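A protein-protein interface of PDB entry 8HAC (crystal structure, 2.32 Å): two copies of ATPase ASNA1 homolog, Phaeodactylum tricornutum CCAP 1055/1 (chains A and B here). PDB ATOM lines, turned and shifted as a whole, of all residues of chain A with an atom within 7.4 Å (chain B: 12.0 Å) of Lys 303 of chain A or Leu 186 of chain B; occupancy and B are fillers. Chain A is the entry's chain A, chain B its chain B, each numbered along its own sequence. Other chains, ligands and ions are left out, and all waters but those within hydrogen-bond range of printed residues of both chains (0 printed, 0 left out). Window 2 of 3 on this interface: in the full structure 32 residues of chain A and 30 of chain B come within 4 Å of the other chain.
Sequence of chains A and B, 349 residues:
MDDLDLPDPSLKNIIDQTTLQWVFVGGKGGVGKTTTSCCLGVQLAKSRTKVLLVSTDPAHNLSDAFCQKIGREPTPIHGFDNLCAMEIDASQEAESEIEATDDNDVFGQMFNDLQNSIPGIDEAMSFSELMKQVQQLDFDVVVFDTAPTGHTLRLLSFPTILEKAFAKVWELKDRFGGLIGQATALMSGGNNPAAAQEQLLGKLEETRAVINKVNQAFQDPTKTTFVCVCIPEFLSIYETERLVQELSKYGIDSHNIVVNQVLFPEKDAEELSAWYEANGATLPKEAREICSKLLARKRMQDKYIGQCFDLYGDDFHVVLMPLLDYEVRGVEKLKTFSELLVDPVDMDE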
ATOM      1  N   PRO A 232     -31.129  -7.142  -1.527  1.00  0.00           N
ATOM      2  CA  PRO A 232     -30.502  -8.094  -0.593  1.00  0.00           C
ATOM      3  C   PRO A 232     -29.659  -9.144  -1.296  1.00  0.00           C
ATOM      4  O   PRO A 232     -29.981 -10.336  -1.245  1.00  0.00           O
ATOM      5  CB  PRO A 232     -31.703  -8.731   0.119  1.00  0.00           C
ATOM      6  CG  PRO A 232     -32.858  -7.811  -0.138  1.00  0.00           C
ATOM      7  CD  PRO A 232     -32.598  -7.229  -1.488  1.00  0.00           C
ATOM      8  N   PHE A 234     -25.270 -10.060  -2.509  1.00  0.00           N
ATOM      9  CA  PHE A 234     -23.899  -9.714  -2.138  1.00  0.00           C
ATOM     10  C   PHE A 234     -23.340  -8.595  -3.012  1.00  0.00           C
ATOM     11  O   PHE A 234     -22.769  -7.627  -2.501  1.00  0.00           O
ATOM     12  CB  PHE A 234     -22.969 -10.926  -2.203  1.00  0.00           C
ATOM     13  CG  PHE A 234     -21.512 -10.541  -2.241  1.00  0.00           C
ATOM     14  CD1 PHE A 234     -20.929  -9.890  -1.162  1.00  0.00           C
ATOM     15  CD2 PHE A 234     -20.739 -10.787  -3.358  1.00  0.00           C
ATOM     16  CE1 PHE A 234     -19.599  -9.504  -1.193  1.00  0.00           C
ATOM     17  CE2 PHE A 234     -19.404 -10.408  -3.394  1.00  0.00           C
ATOM     18  CZ  PHE A 234     -18.834  -9.768  -2.308  1.00  0.00           C
ATOM     19  N   ILE A 237     -24.697  -5.057  -2.291  1.00  0.00           N
ATOM     20  CA  ILE A 237     -24.208  -4.515  -1.029  1.00  0.00           C
ATOM     21  C   ILE A 237     -22.735  -4.158  -1.137  1.00  0.00           C
ATOM     22  O   ILE A 237     -22.278  -3.169  -0.546  1.00  0.00           O
ATOM     23  CB  ILE A 237     -24.475  -5.535   0.096  1.00  0.00           C
ATOM     24  CG1 ILE A 237     -25.983  -5.745   0.274  1.00  0.00           C
ATOM     25  CG2 ILE A 237     -23.806  -5.117   1.397  1.00  0.00           C
ATOM     26  CD1 ILE A 237     -26.318  -6.826   1.276  1.00  0.00           C
ATOM     27  N   ARG A 297     -34.968 -18.240  -1.182  1.00  0.00           N
ATOM     28  CA  ARG A 297     -34.663 -16.842  -1.482  1.00  0.00           C
ATOM     29  C   ARG A 297     -34.789 -15.964  -0.243  1.00  0.00           C
ATOM     30  O   ARG A 297     -33.972 -15.060  -0.031  1.00  0.00           O
ATOM     31  CB  ARG A 297     -35.558 -16.288  -2.589  1.00  0.00           C
ATOM     32  CG  ARG A 297     -35.271 -16.785  -3.983  1.00  0.00           C
ATOM     33  CD  ARG A 297     -36.034 -15.932  -4.972  1.00  0.00           C
ATOM     34  NE  ARG A 297     -35.649 -14.533  -4.797  1.00  0.00           N
ATOM     35  CZ  ARG A 297     -36.304 -13.490  -5.287  1.00  0.00           C
ATOM     36  NH1 ARG A 297     -37.407 -13.637  -6.002  1.00  0.00           N
ATOM     37  NH2 ARG A 297     -35.841 -12.266  -5.047  1.00  0.00           N
ATOM     38  N   LYS A 298     -35.814 -16.206   0.583  1.00  0.00           N
ATOM     39  CA  LYS A 298     -36.008 -15.377   1.766  1.00  0.00           C
ATOM     40  C   LYS A 298     -34.863 -15.553   2.755  1.00  0.00           C
ATOM     41  O   LYS A 298     -34.380 -14.571   3.329  1.00  0.00           O
ATOM     42  CB  LYS A 298     -37.351 -15.699   2.418  1.00  0.00           C
ATOM     43  CG  LYS A 298     -37.606 -14.949   3.710  1.00  0.00           C
ATOM     44  CD  LYS A 298     -37.846 -13.472   3.419  1.00  0.00           C
ATOM     45  CE  LYS A 298     -38.723 -12.818   4.465  1.00  0.00           C
ATOM     46  NZ  LYS A 298     -40.166 -13.107   4.202  1.00  0.00           N
ATOM     47  N   ARG A 299     -34.406 -16.794   2.950  1.00  0.00           N
ATOM     48  CA  ARG A 299     -33.270 -17.038   3.835  1.00  0.00           C
ATOM     49  C   ARG A 299     -32.031 -16.281   3.359  1.00  0.00           C
ATOM     50  O   ARG A 299     -31.344 -15.614   4.154  1.00  0.00           O
ATOM     51  CB  ARG A 299     -32.985 -18.539   3.908  1.00  0.00           C
ATOM     52  CG  ARG A 299     -33.975 -19.347   4.732  1.00  0.00           C
ATOM     53  CD  ARG A 299     -33.464 -20.769   4.909  1.00  0.00           C
ATOM     54  NE  ARG A 299     -33.263 -21.421   3.620  1.00  0.00           N
ATOM     55  CZ  ARG A 299     -33.899 -22.514   3.219  1.00  0.00           C
ATOM     56  NH1 ARG A 299     -34.775 -23.129   3.998  1.00  0.00           N
ATOM     57  NH2 ARG A 299     -33.655 -22.999   2.005  1.00  0.00           N
ATOM     58  N   MET A 300     -31.739 -16.365   2.053  1.00  0.00           N
ATOM     59  CA  MET A 300     -30.582 -15.654   1.501  1.00  0.00           C
ATOM     60  C   MET A 300     -30.718 -14.141   1.682  1.00  0.00           C
ATOM     61  O   MET A 300     -29.786 -13.458   2.149  1.00  0.00           O
ATOM     62  CB  MET A 300     -30.430 -16.007   0.019  1.00  0.00           C
ATOM     63  CG  MET A 300     -29.059 -15.715  -0.577  1.00  0.00           C
ATOM     64  SD  MET A 300     -27.780 -16.897  -0.118  1.00  0.00           S
ATOM     65  CE  MET A 300     -28.140 -18.225  -1.267  1.00  0.00           C
ATOM     66  N   GLN A 301     -31.884 -13.599   1.314  1.00  0.00           N
ATOM     67  CA  GLN A 301     -32.133 -12.171   1.461  1.00  0.00           C
ATOM     68  C   GLN A 301     -31.979 -11.725   2.906  1.00  0.00           C
ATOM     69  O   GLN A 301     -31.485 -10.624   3.165  1.00  0.00           O
ATOM     70  CB  GLN A 301     -33.530 -11.826   0.945  1.00  0.00           C
ATOM     71  CG  GLN A 301     -33.630 -11.760  -0.566  1.00  0.00           C
ATOM     72  CD  GLN A 301     -34.825 -10.951  -1.031  1.00  0.00           C
ATOM     73  OE1 GLN A 301     -35.577 -10.411  -0.219  1.00  0.00           O
ATOM     74  NE2 GLN A 301     -34.992 -10.841  -2.343  1.00  0.00           N
ATOM     75  N   ASP A 302     -32.410 -12.557   3.860  1.00  0.00           N
ATOM     76  CA  ASP A 302     -32.292 -12.190   5.268  1.00  0.00           C
ATOM     77  C   ASP A 302     -30.840 -12.133   5.706  1.00  0.00           C
ATOM     78  O   ASP A 302     -30.456 -11.248   6.484  1.00  0.00           O
ATOM     79  CB  ASP A 302     -33.069 -13.169   6.148  1.00  0.00           C
ATOM     80  CG  ASP A 302     -34.533 -12.819   6.247  1.00  0.00           C
ATOM     81  OD1 ASP A 302     -34.930 -11.753   5.721  1.00  0.00           O
ATOM     82  OD2 ASP A 302     -35.288 -13.609   6.852  1.00  0.00           O
ATOM     83  N   LYS A 303     -30.017 -13.076   5.241  1.00  0.00           N
ATOM     84  CA  LYS A 303     -28.585 -12.947   5.502  1.00  0.00           C
ATOM     85  C   LYS A 303     -28.055 -11.607   5.011  1.00  0.00           C
ATOM     86  O   LYS A 303     -27.359 -10.888   5.743  1.00  0.00           O
ATOM     87  CB  LYS A 303     -27.811 -14.107   4.878  1.00  0.00           C
ATOM     88  CG  LYS A 303     -27.931 -15.376   5.690  1.00  0.00           C
ATOM     89  CD  LYS A 303     -27.453 -15.067   7.110  1.00  0.00           C
ATOM     90  CE  LYS A 303     -26.874 -16.273   7.818  1.00  0.00           C
ATOM     91  NZ  LYS A 303     -26.021 -15.858   8.970  1.00  0.00           N
ATOM     92  N   TYR A 304     -28.409 -11.230   3.781  1.00  0.00           N
ATOM     93  CA  TYR A 304     -27.830  -9.993   3.257  1.00  0.00           C
ATOM     94  C   TYR A 304     -28.424  -8.745   3.914  1.00  0.00           C
ATOM     95  O   TYR A 304     -27.729  -7.735   4.067  1.00  0.00           O
ATOM     96  CB  TYR A 304     -27.959  -9.959   1.739  1.00  0.00           C
ATOM     97  CG  TYR A 304     -26.981 -10.929   1.110  1.00  0.00           C
ATOM     98  CD1 TYR A 304     -25.615 -10.781   1.305  1.00  0.00           C
ATOM     99  CD2 TYR A 304     -27.423 -12.000   0.347  1.00  0.00           C
ATOM    100  CE1 TYR A 304     -24.713 -11.670   0.750  1.00  0.00           C
ATOM    101  CE2 TYR A 304     -26.531 -12.892  -0.216  1.00  0.00           C
ATOM    102  CZ  TYR A 304     -25.175 -12.722  -0.009  1.00  0.00           C
ATOM    103  OH  TYR A 304     -24.281 -13.606  -0.568  1.00  0.00           O
ATOM    104  N   ILE A 305     -29.679  -8.801   4.356  1.00  0.00           N
ATOM    105  CA  ILE A 305     -30.267  -7.661   5.056  1.00  0.00           C
ATOM    106  C   ILE A 305     -29.636  -7.503   6.434  1.00  0.00           C
ATOM    107  O   ILE A 305     -29.417  -6.379   6.911  1.00  0.00           O
ATOM    108  CB  ILE A 305     -31.799  -7.819   5.130  1.00  0.00           C
ATOM    109  CG1 ILE A 305     -32.425  -7.591   3.751  1.00  0.00           C
ATOM    110  CG2 ILE A 305     -32.398  -6.870   6.155  1.00  0.00           C
ATOM    111  CD1 ILE A 305     -33.771  -8.250   3.564  1.00  0.00           C
ATOM    112  N   GLY A 306     -29.318  -8.621   7.091  1.00  0.00           N
ATOM    113  CA  GLY A 306     -28.540  -8.541   8.317  1.00  0.00           C
ATOM    114  C   GLY A 306     -27.168  -7.939   8.084  1.00  0.00           C
ATOM    115  O   GLY A 306     -26.674  -7.158   8.899  1.00  0.00           O
ATOM    116  N   GLN A 307     -26.543  -8.283   6.954  1.00  0.00           N
ATOM    117  CA  GLN A 307     -25.274  -7.652   6.593  1.00  0.00           C
ATOM    118  C   GLN A 307     -25.439  -6.143   6.426  1.00  0.00           C
ATOM    119  O   GLN A 307     -24.591  -5.361   6.879  1.00  0.00           O
ATOM    120  CB  GLN A 307     -24.734  -8.283   5.308  1.00  0.00           C
ATOM    121  CG  GLN A 307     -23.220  -8.331   5.200  1.00  0.00           C
ATOM    122  CD  GLN A 307     -22.742  -9.414   4.245  1.00  0.00           C
ATOM    123  OE1 GLN A 307     -22.274 -10.468   4.673  1.00  0.00           O
ATOM    124  NE2 GLN A 307     -22.861  -9.160   2.946  1.00  0.00           N
ATOM    125  N   CYS A 308     -26.534  -5.721   5.783  1.00  0.00           N
ATOM    126  CA  CYS A 308     -26.826  -4.295   5.623  1.00  0.00           C
ATOM    127  C   CYS A 308     -26.940  -3.602   6.969  1.00  0.00           C
ATOM    128  O   CYS A 308     -26.400  -2.508   7.169  1.00  0.00           O
ATOM    129  CB  CYS A 308     -28.125  -4.093   4.845  1.00  0.00           C
ATOM    130  SG  CYS A 308     -28.019  -4.334   3.080  1.00  0.00           S
ATOM    131  N   PHE A 309     -27.676  -4.208   7.897  1.00  0.00           N
ATOM    132  CA  PHE A 309     -27.830  -3.588   9.207  1.00  0.00           C
ATOM    133  C   PHE A 309     -26.537  -3.625  10.009  1.00  0.00           C
ATOM    134  O   PHE A 309     -26.340  -2.779  10.885  1.00  0.00           O
ATOM    135  CB  PHE A 309     -28.967  -4.253   9.981  1.00  0.00           C
ATOM    136  CG  PHE A 309     -30.319  -3.653   9.701  1.00  0.00           C
ATOM    137  CD1 PHE A 309     -30.691  -2.449  10.285  1.00  0.00           C
ATOM    138  CD2 PHE A 309     -31.213  -4.289   8.854  1.00  0.00           C
ATOM    139  CE1 PHE A 309     -31.936  -1.891  10.032  1.00  0.00           C
ATOM    140  CE2 PHE A 309     -32.463  -3.741   8.598  1.00  0.00           C
ATOM    141  CZ  PHE A 309     -32.826  -2.541   9.186  1.00  0.00           C
ATOM    142  N   ASP A 310     -25.647  -4.577   9.723  1.00  0.00           N
ATOM    143  CA  ASP A 310     -24.323  -4.550  10.340  1.00  0.00           C
ATOM    144  C   ASP A 310     -23.518  -3.361   9.832  1.00  0.00           C
ATOM    145  O   ASP A 310     -22.949  -2.599  10.624  1.00  0.00           O
ATOM    146  CB  ASP A 310     -23.578  -5.855  10.058  1.00  0.00           C
ATOM    147  CG  ASP A 310     -24.148  -7.030  10.819  1.00  0.00           C
ATOM    148  OD1 ASP A 310     -24.775  -6.808  11.876  1.00  0.00           O
ATOM    149  OD2 ASP A 310     -23.966  -8.179  10.357  1.00  0.00           O
ATOM    150  N   ASN B 104     -24.581 -12.850  -8.492  1.00  0.00           N
ATOM    151  CA  ASN B 104     -23.985 -13.761  -9.464  1.00  0.00           C
ATOM    152  C   ASN B 104     -22.457 -13.654  -9.472  1.00  0.00           C
ATOM    153  O   ASN B 104     -21.825 -13.675  -8.416  1.00  0.00           O
ATOM    154  CB  ASN B 104     -24.558 -13.539 -10.872  1.00  0.00           C
ATOM    155  CG  ASN B 104     -24.601 -12.080 -11.277  1.00  0.00           C
ATOM    156  OD1 ASN B 104     -23.690 -11.583 -11.940  1.00  0.00           O
ATOM    157  ND2 ASN B 104     -25.674 -11.391 -10.902  1.00  0.00           N
ATOM    158  N   VAL B 106     -18.940 -12.909  -9.119  1.00  0.00           N
ATOM    159  CA  VAL B 106     -18.163 -11.934  -8.361  1.00  0.00           C
ATOM    160  C   VAL B 106     -16.943 -11.484  -9.150  1.00  0.00           C
ATOM    161  O   VAL B 106     -16.593 -10.294  -9.158  1.00  0.00           O
ATOM    162  CB  VAL B 106     -17.756 -12.529  -7.003  1.00  0.00           C
ATOM    163  CG1 VAL B 106     -16.873 -11.556  -6.241  1.00  0.00           C
ATOM    164  CG2 VAL B 106     -18.989 -12.909  -6.197  1.00  0.00           C
ATOM    165  N   GLY B 177     -11.873  -6.010   2.861  1.00  0.00           N
ATOM    166  CA  GLY B 177     -11.608  -7.366   3.315  1.00  0.00           C
ATOM    167  C   GLY B 177     -12.659  -7.897   4.267  1.00  0.00           C
ATOM    168  O   GLY B 177     -13.011  -9.077   4.218  1.00  0.00           O
ATOM    169  N   GLY B 178     -13.161  -7.045   5.156  1.00  0.00           N
ATOM    170  CA  GLY B 178     -14.204  -7.454   6.077  1.00  0.00           C
ATOM    171  C   GLY B 178     -15.440  -7.976   5.376  1.00  0.00           C
ATOM    172  O   GLY B 178     -15.878  -9.107   5.625  1.00  0.00           O
ATOM    173  N   LEU B 179     -16.009  -7.153   4.491  1.00  0.00           N
ATOM    174  CA  LEU B 179     -17.189  -7.563   3.735  1.00  0.00           C
ATOM    175  C   LEU B 179     -16.903  -8.798   2.888  1.00  0.00           C
ATOM    176  O   LEU B 179     -17.736  -9.711   2.810  1.00  0.00           O
ATOM    177  CB  LEU B 179     -17.675  -6.405   2.860  1.00  0.00           C
ATOM    178  CG  LEU B 179     -18.884  -6.633   1.947  1.00  0.00           C
ATOM    179  CD1 LEU B 179     -20.037  -7.277   2.703  1.00  0.00           C
ATOM    180  CD2 LEU B 179     -19.325  -5.328   1.293  1.00  0.00           C
ATOM    181  N   ILE B 180     -15.726  -8.853   2.257  1.00  0.00           N
ATOM    182  CA  ILE B 180     -15.411  -9.964   1.362  1.00  0.00           C
ATOM    183  C   ILE B 180     -15.327 -11.275   2.140  1.00  0.00           C
ATOM    184  O   ILE B 180     -15.881 -12.303   1.725  1.00  0.00           O
ATOM    185  CB  ILE B 180     -14.110  -9.668   0.589  1.00  0.00           C
ATOM    186  CG1 ILE B 180     -14.375  -8.672  -0.545  1.00  0.00           C
ATOM    187  CG2 ILE B 180     -13.488 -10.949   0.052  1.00  0.00           C
ATOM    188  CD1 ILE B 180     -13.137  -8.298  -1.333  1.00  0.00           C
ATOM    189  N   GLY B 181     -14.641 -11.258   3.287  1.00  0.00           N
ATOM    190  CA  GLY B 181     -14.559 -12.454   4.108  1.00  0.00           C
ATOM    191  C   GLY B 181     -15.897 -12.857   4.697  1.00  0.00           C
ATOM    192  O   GLY B 181     -16.213 -14.048   4.785  1.00  0.00           O
ATOM    193  N   GLN B 182     -16.702 -11.875   5.116  1.00  0.00           N
ATOM    194  CA  GLN B 182     -18.023 -12.180   5.654  1.00  0.00           C
ATOM    195  C   GLN B 182     -18.927 -12.808   4.600  1.00  0.00           C
ATOM    196  O   GLN B 182     -19.762 -13.661   4.924  1.00  0.00           O
ATOM    197  CB  GLN B 182     -18.659 -10.906   6.212  1.00  0.00           C
ATOM    198  CG  GLN B 182     -19.988 -11.113   6.919  1.00  0.00           C
ATOM    199  CD  GLN B 182     -20.488  -9.849   7.592  1.00  0.00           C
ATOM    200  OE1 GLN B 182     -19.844  -8.801   7.523  1.00  0.00           O
ATOM    201  NE2 GLN B 182     -21.643  -9.940   8.244  1.00  0.00           N
ATOM    202  N   ALA B 183     -18.773 -12.402   3.337  1.00  0.00           N
ATOM    203  CA  ALA B 183     -19.561 -12.975   2.251  1.00  0.00           C
ATOM    204  C   ALA B 183     -19.044 -14.330   1.780  1.00  0.00           C
ATOM    205  O   ALA B 183     -19.826 -15.131   1.255  1.00  0.00           O
ATOM    206  CB  ALA B 183     -19.603 -12.008   1.073  1.00  0.00           C
ATOM    207  N   THR B 184     -17.741 -14.592   1.929  1.00  0.00           N
ATOM    208  CA  THR B 184     -17.184 -15.870   1.485  1.00  0.00           C
ATOM    209  C   THR B 184     -17.899 -17.058   2.130  1.00  0.00           C
ATOM    210  O   THR B 184     -18.121 -18.086   1.477  1.00  0.00           O
ATOM    211  CB  THR B 184     -15.681 -15.912   1.786  1.00  0.00           C
ATOM    212  OG1 THR B 184     -14.989 -15.003   0.918  1.00  0.00           O
ATOM    213  CG2 THR B 184     -15.117 -17.318   1.588  1.00  0.00           C
ATOM    214  N   ALA B 185     -18.282 -16.931   3.401  1.00  0.00           N
ATOM    215  CA  ALA B 185     -18.971 -18.024   4.080  1.00  0.00           C
ATOM    216  C   ALA B 185     -20.315 -18.358   3.437  1.00  0.00           C
ATOM    217  O   ALA B 185     -20.732 -19.523   3.449  1.00  0.00           O
ATOM    218  CB  ALA B 185     -19.167 -17.681   5.557  1.00  0.00           C
ATOM    219  N   LEU B 186     -21.006 -17.365   2.878  1.00  0.00           N
ATOM    220  CA  LEU B 186     -22.357 -17.590   2.356  1.00  0.00           C
ATOM    221  C   LEU B 186     -22.354 -18.266   0.987  1.00  0.00           C
ATOM    222  O   LEU B 186     -22.772 -19.420   0.847  1.00  0.00           O
ATOM    223  CB  LEU B 186     -23.122 -16.262   2.295  1.00  0.00           C
ATOM    224  CG  LEU B 186     -23.707 -15.737   3.607  1.00  0.00           C
ATOM    225  CD1 LEU B 186     -24.269 -14.335   3.423  1.00  0.00           C
ATOM    226  CD2 LEU B 186     -24.776 -16.683   4.128  1.00  0.00           C
ATOM    227  N   MET B 187     -21.886 -17.553  -0.035  1.00  0.00           N
ATOM    228  CA  MET B 187     -21.970 -18.030  -1.412  1.00  0.00           C
ATOM    229  C   MET B 187     -20.999 -19.179  -1.668  1.00  0.00           C
ATOM    230  O   MET B 187     -19.788 -19.044  -1.466  1.00  0.00           O
ATOM    231  CB  MET B 187     -21.709 -16.873  -2.371  1.00  0.00           C
ATOM    232  CG  MET B 187     -20.487 -16.043  -2.023  1.00  0.00           C
ATOM    233  SD  MET B 187     -20.751 -14.305  -2.405  1.00  0.00           S
ATOM    234  CE  MET B 187     -21.405 -14.422  -4.069  1.00  0.00           C
ATOM    235  N   SER B 188     -21.539 -20.310  -2.112  1.00  0.00           N
ATOM    236  CA  SER B 188     -20.767 -21.507  -2.396  1.00  0.00           C
ATOM    237  C   SER B 188     -20.500 -21.630  -3.894  1.00  0.00           C
ATOM    238  O   SER B 188     -21.011 -20.863  -4.715  1.00  0.00           O
ATOM    239  CB  SER B 188     -21.495 -22.753  -1.880  1.00  0.00           C
ATOM    240  OG  SER B 188     -21.645 -22.717  -0.471  1.00  0.00           O
ATOM    241  N   GLY B 189     -19.682 -22.621  -4.240  1.00  0.00           N
ATOM    242  CA  GLY B 189     -19.321 -22.848  -5.631  1.00  0.00           C
ATOM    243  C   GLY B 189     -18.419 -21.767  -6.197  1.00  0.00           C
ATOM    244  O   GLY B 189     -17.469 -21.309  -5.552  1.00  0.00           O
ATOM    245  N   GLY B 190     -18.720 -21.358  -7.429  1.00  0.00           N
ATOM    246  CA  GLY B 190     -17.900 -20.415  -8.167  1.00  0.00           C
ATOM    247  C   GLY B 190     -18.118 -18.936  -7.936  1.00  0.00           C
ATOM    248  O   GLY B 190     -18.207 -18.174  -8.904  1.00  0.00           O
ATOM    249  N   ASN B 191     -18.191 -18.502  -6.672  1.00  0.00           N
ATOM    250  CA  ASN B 191     -18.406 -17.085  -6.392  1.00  0.00           C
ATOM    251  C   ASN B 191     -17.782 -16.653  -5.070  1.00  0.00           C
ATOM    252  O   ASN B 191     -18.266 -15.708  -4.438  1.00  0.00           O
ATOM    253  CB  ASN B 191     -19.896 -16.729  -6.417  1.00  0.00           C
ATOM    254  CG  ASN B 191     -20.422 -16.568  -7.828  1.00  0.00           C
ATOM    255  OD1 ASN B 191     -19.899 -15.765  -8.603  1.00  0.00           O
ATOM    256  ND2 ASN B 191     -21.458 -17.323  -8.170  1.00  0.00           N
ATOM    257  N   ASN B 192     -16.743 -17.343  -4.631  1.00  0.00           N
ATOM    258  CA  ASN B 192     -15.973 -16.902  -3.481  1.00  0.00           C
ATOM    259  C   ASN B 192     -15.359 -15.541  -3.799  1.00  0.00           C
ATOM    260  O   ASN B 192     -14.585 -15.431  -4.764  1.00  0.00           O
ATOM    261  CB  ASN B 192     -14.892 -17.931  -3.156  1.00  0.00           C
ATOM    262  CG  ASN B 192     -14.092 -17.583  -1.913  1.00  0.00           C
ATOM    263  OD1 ASN B 192     -14.135 -16.457  -1.417  1.00  0.00           O
ATOM    264  ND2 ASN B 192     -13.341 -18.558  -1.410  1.00  0.00           N
ATOM    265  N   PRO B 193     -15.688 -14.484  -3.049  1.00  0.00           N
ATOM    266  CA  PRO B 193     -15.112 -13.164  -3.361  1.00  0.00           C
ATOM    267  C   PRO B 193     -13.600 -13.107  -3.221  1.00  0.00           C
ATOM    268  O   PRO B 193     -12.932 -12.489  -4.061  1.00  0.00           O
ATOM    269  CB  PRO B 193     -15.808 -12.233  -2.356  1.00  0.00           C
ATOM    270  CG  PRO B 193     -17.057 -12.949  -1.969  1.00  0.00           C
ATOM    271  CD  PRO B 193     -16.708 -14.408  -1.989  1.00  0.00           C
ATOM    272  N   ALA B 194     -13.036 -13.728  -2.182  1.00  0.00           N
ATOM    273  CA  ALA B 194     -11.586 -13.722  -2.016  1.00  0.00           C
ATOM    274  C   ALA B 194     -10.897 -14.463  -3.157  1.00  0.00           C
ATOM    275  O   ALA B 194      -9.858 -14.016  -3.667  1.00  0.00           O
ATOM    276  CB  ALA B 194     -11.207 -14.338  -0.668  1.00  0.00           C
ATOM    277  N   ALA B 195     -11.468 -15.591  -3.579  1.00  0.00           N
ATOM    278  CA  ALA B 195     -10.925 -16.291  -4.735  1.00  0.00           C
ATOM    279  C   ALA B 195     -11.049 -15.441  -5.991  1.00  0.00           C
ATOM    280  O   ALA B 195     -10.146 -15.433  -6.833  1.00  0.00           O
ATOM    281  CB  ALA B 195     -11.629 -17.635  -4.918  1.00  0.00           C
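The backbone carbonyl oxygen (O) of Tyr 304 of chain A lies within hydrogen-bond range of the side-chain sulfur (SG) of Cys 308 of chain A. The side-chain amide oxygen (OD1) of Asn 191 of chain B is in hydrogen-bond range of the backbone NH (N) of Val 106 of chain B.
Among the printed residues, pairs that only touch across the chains: Gln 307 of chain A with Gln 182 of chain B, Phe 234 of chain A with Ala 183 of chain B, Gln 307 of chain A with Leu 179 of chain B, Asp 310 of chain A with Gln 182 of chain B, Phe 234 of chain A with Met 187 of chain B, Phe 234 of chain A with Pro 193 of chain B, Lys 303 of chain A with Leu 186 of chain B, Phe 234 of chain A with Val 106 of chain B and Tyr 304 of chain A with Leu 186 of chain B.
Of chain B, only Leu 186 comes within 4 Å of Lys 303 of chain A. Leu 186 of chain B touches two residues of chain A. No residue of chain B comes within 4 Å of Met 300 of chain A. No residue of chain B comes within 4 Å of Asp 302 of chain A. Tyr 304 of chain A touches just one residue of chain B: Leu 186. No residue of chain B comes within 4 Å of Ile 305 of chain A. Ala 185 of chain B touches none of the printed residues of chain A. Of the printed residues of chain B, Phe 234 of chain A touches Val 106, Ala 183, Met 187 and Pro 193. Printed residues of chain A within 4 Å of Gln 182 of chain B: Gln 307 (3.3 Å) and Asp 310 (3.6 Å). Of the printed residues of chain A, Ala 183 of chain B touches Phe 234 (3.4 Å). Ile 237 of chain A touches none of the printed residues of chain B. The nearest printed residue of chain A that does not touch Val 106 of chain B is Tyr 304 of chain A (7.8 Å).
Of the 17 printed residues of chain A, 5 touch a printed residue of chain B. Hydrophobic or aromatic side chains of chain A that line the printed part of chain B: Phe 234 and Tyr 304.
No position is printed for both chains.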
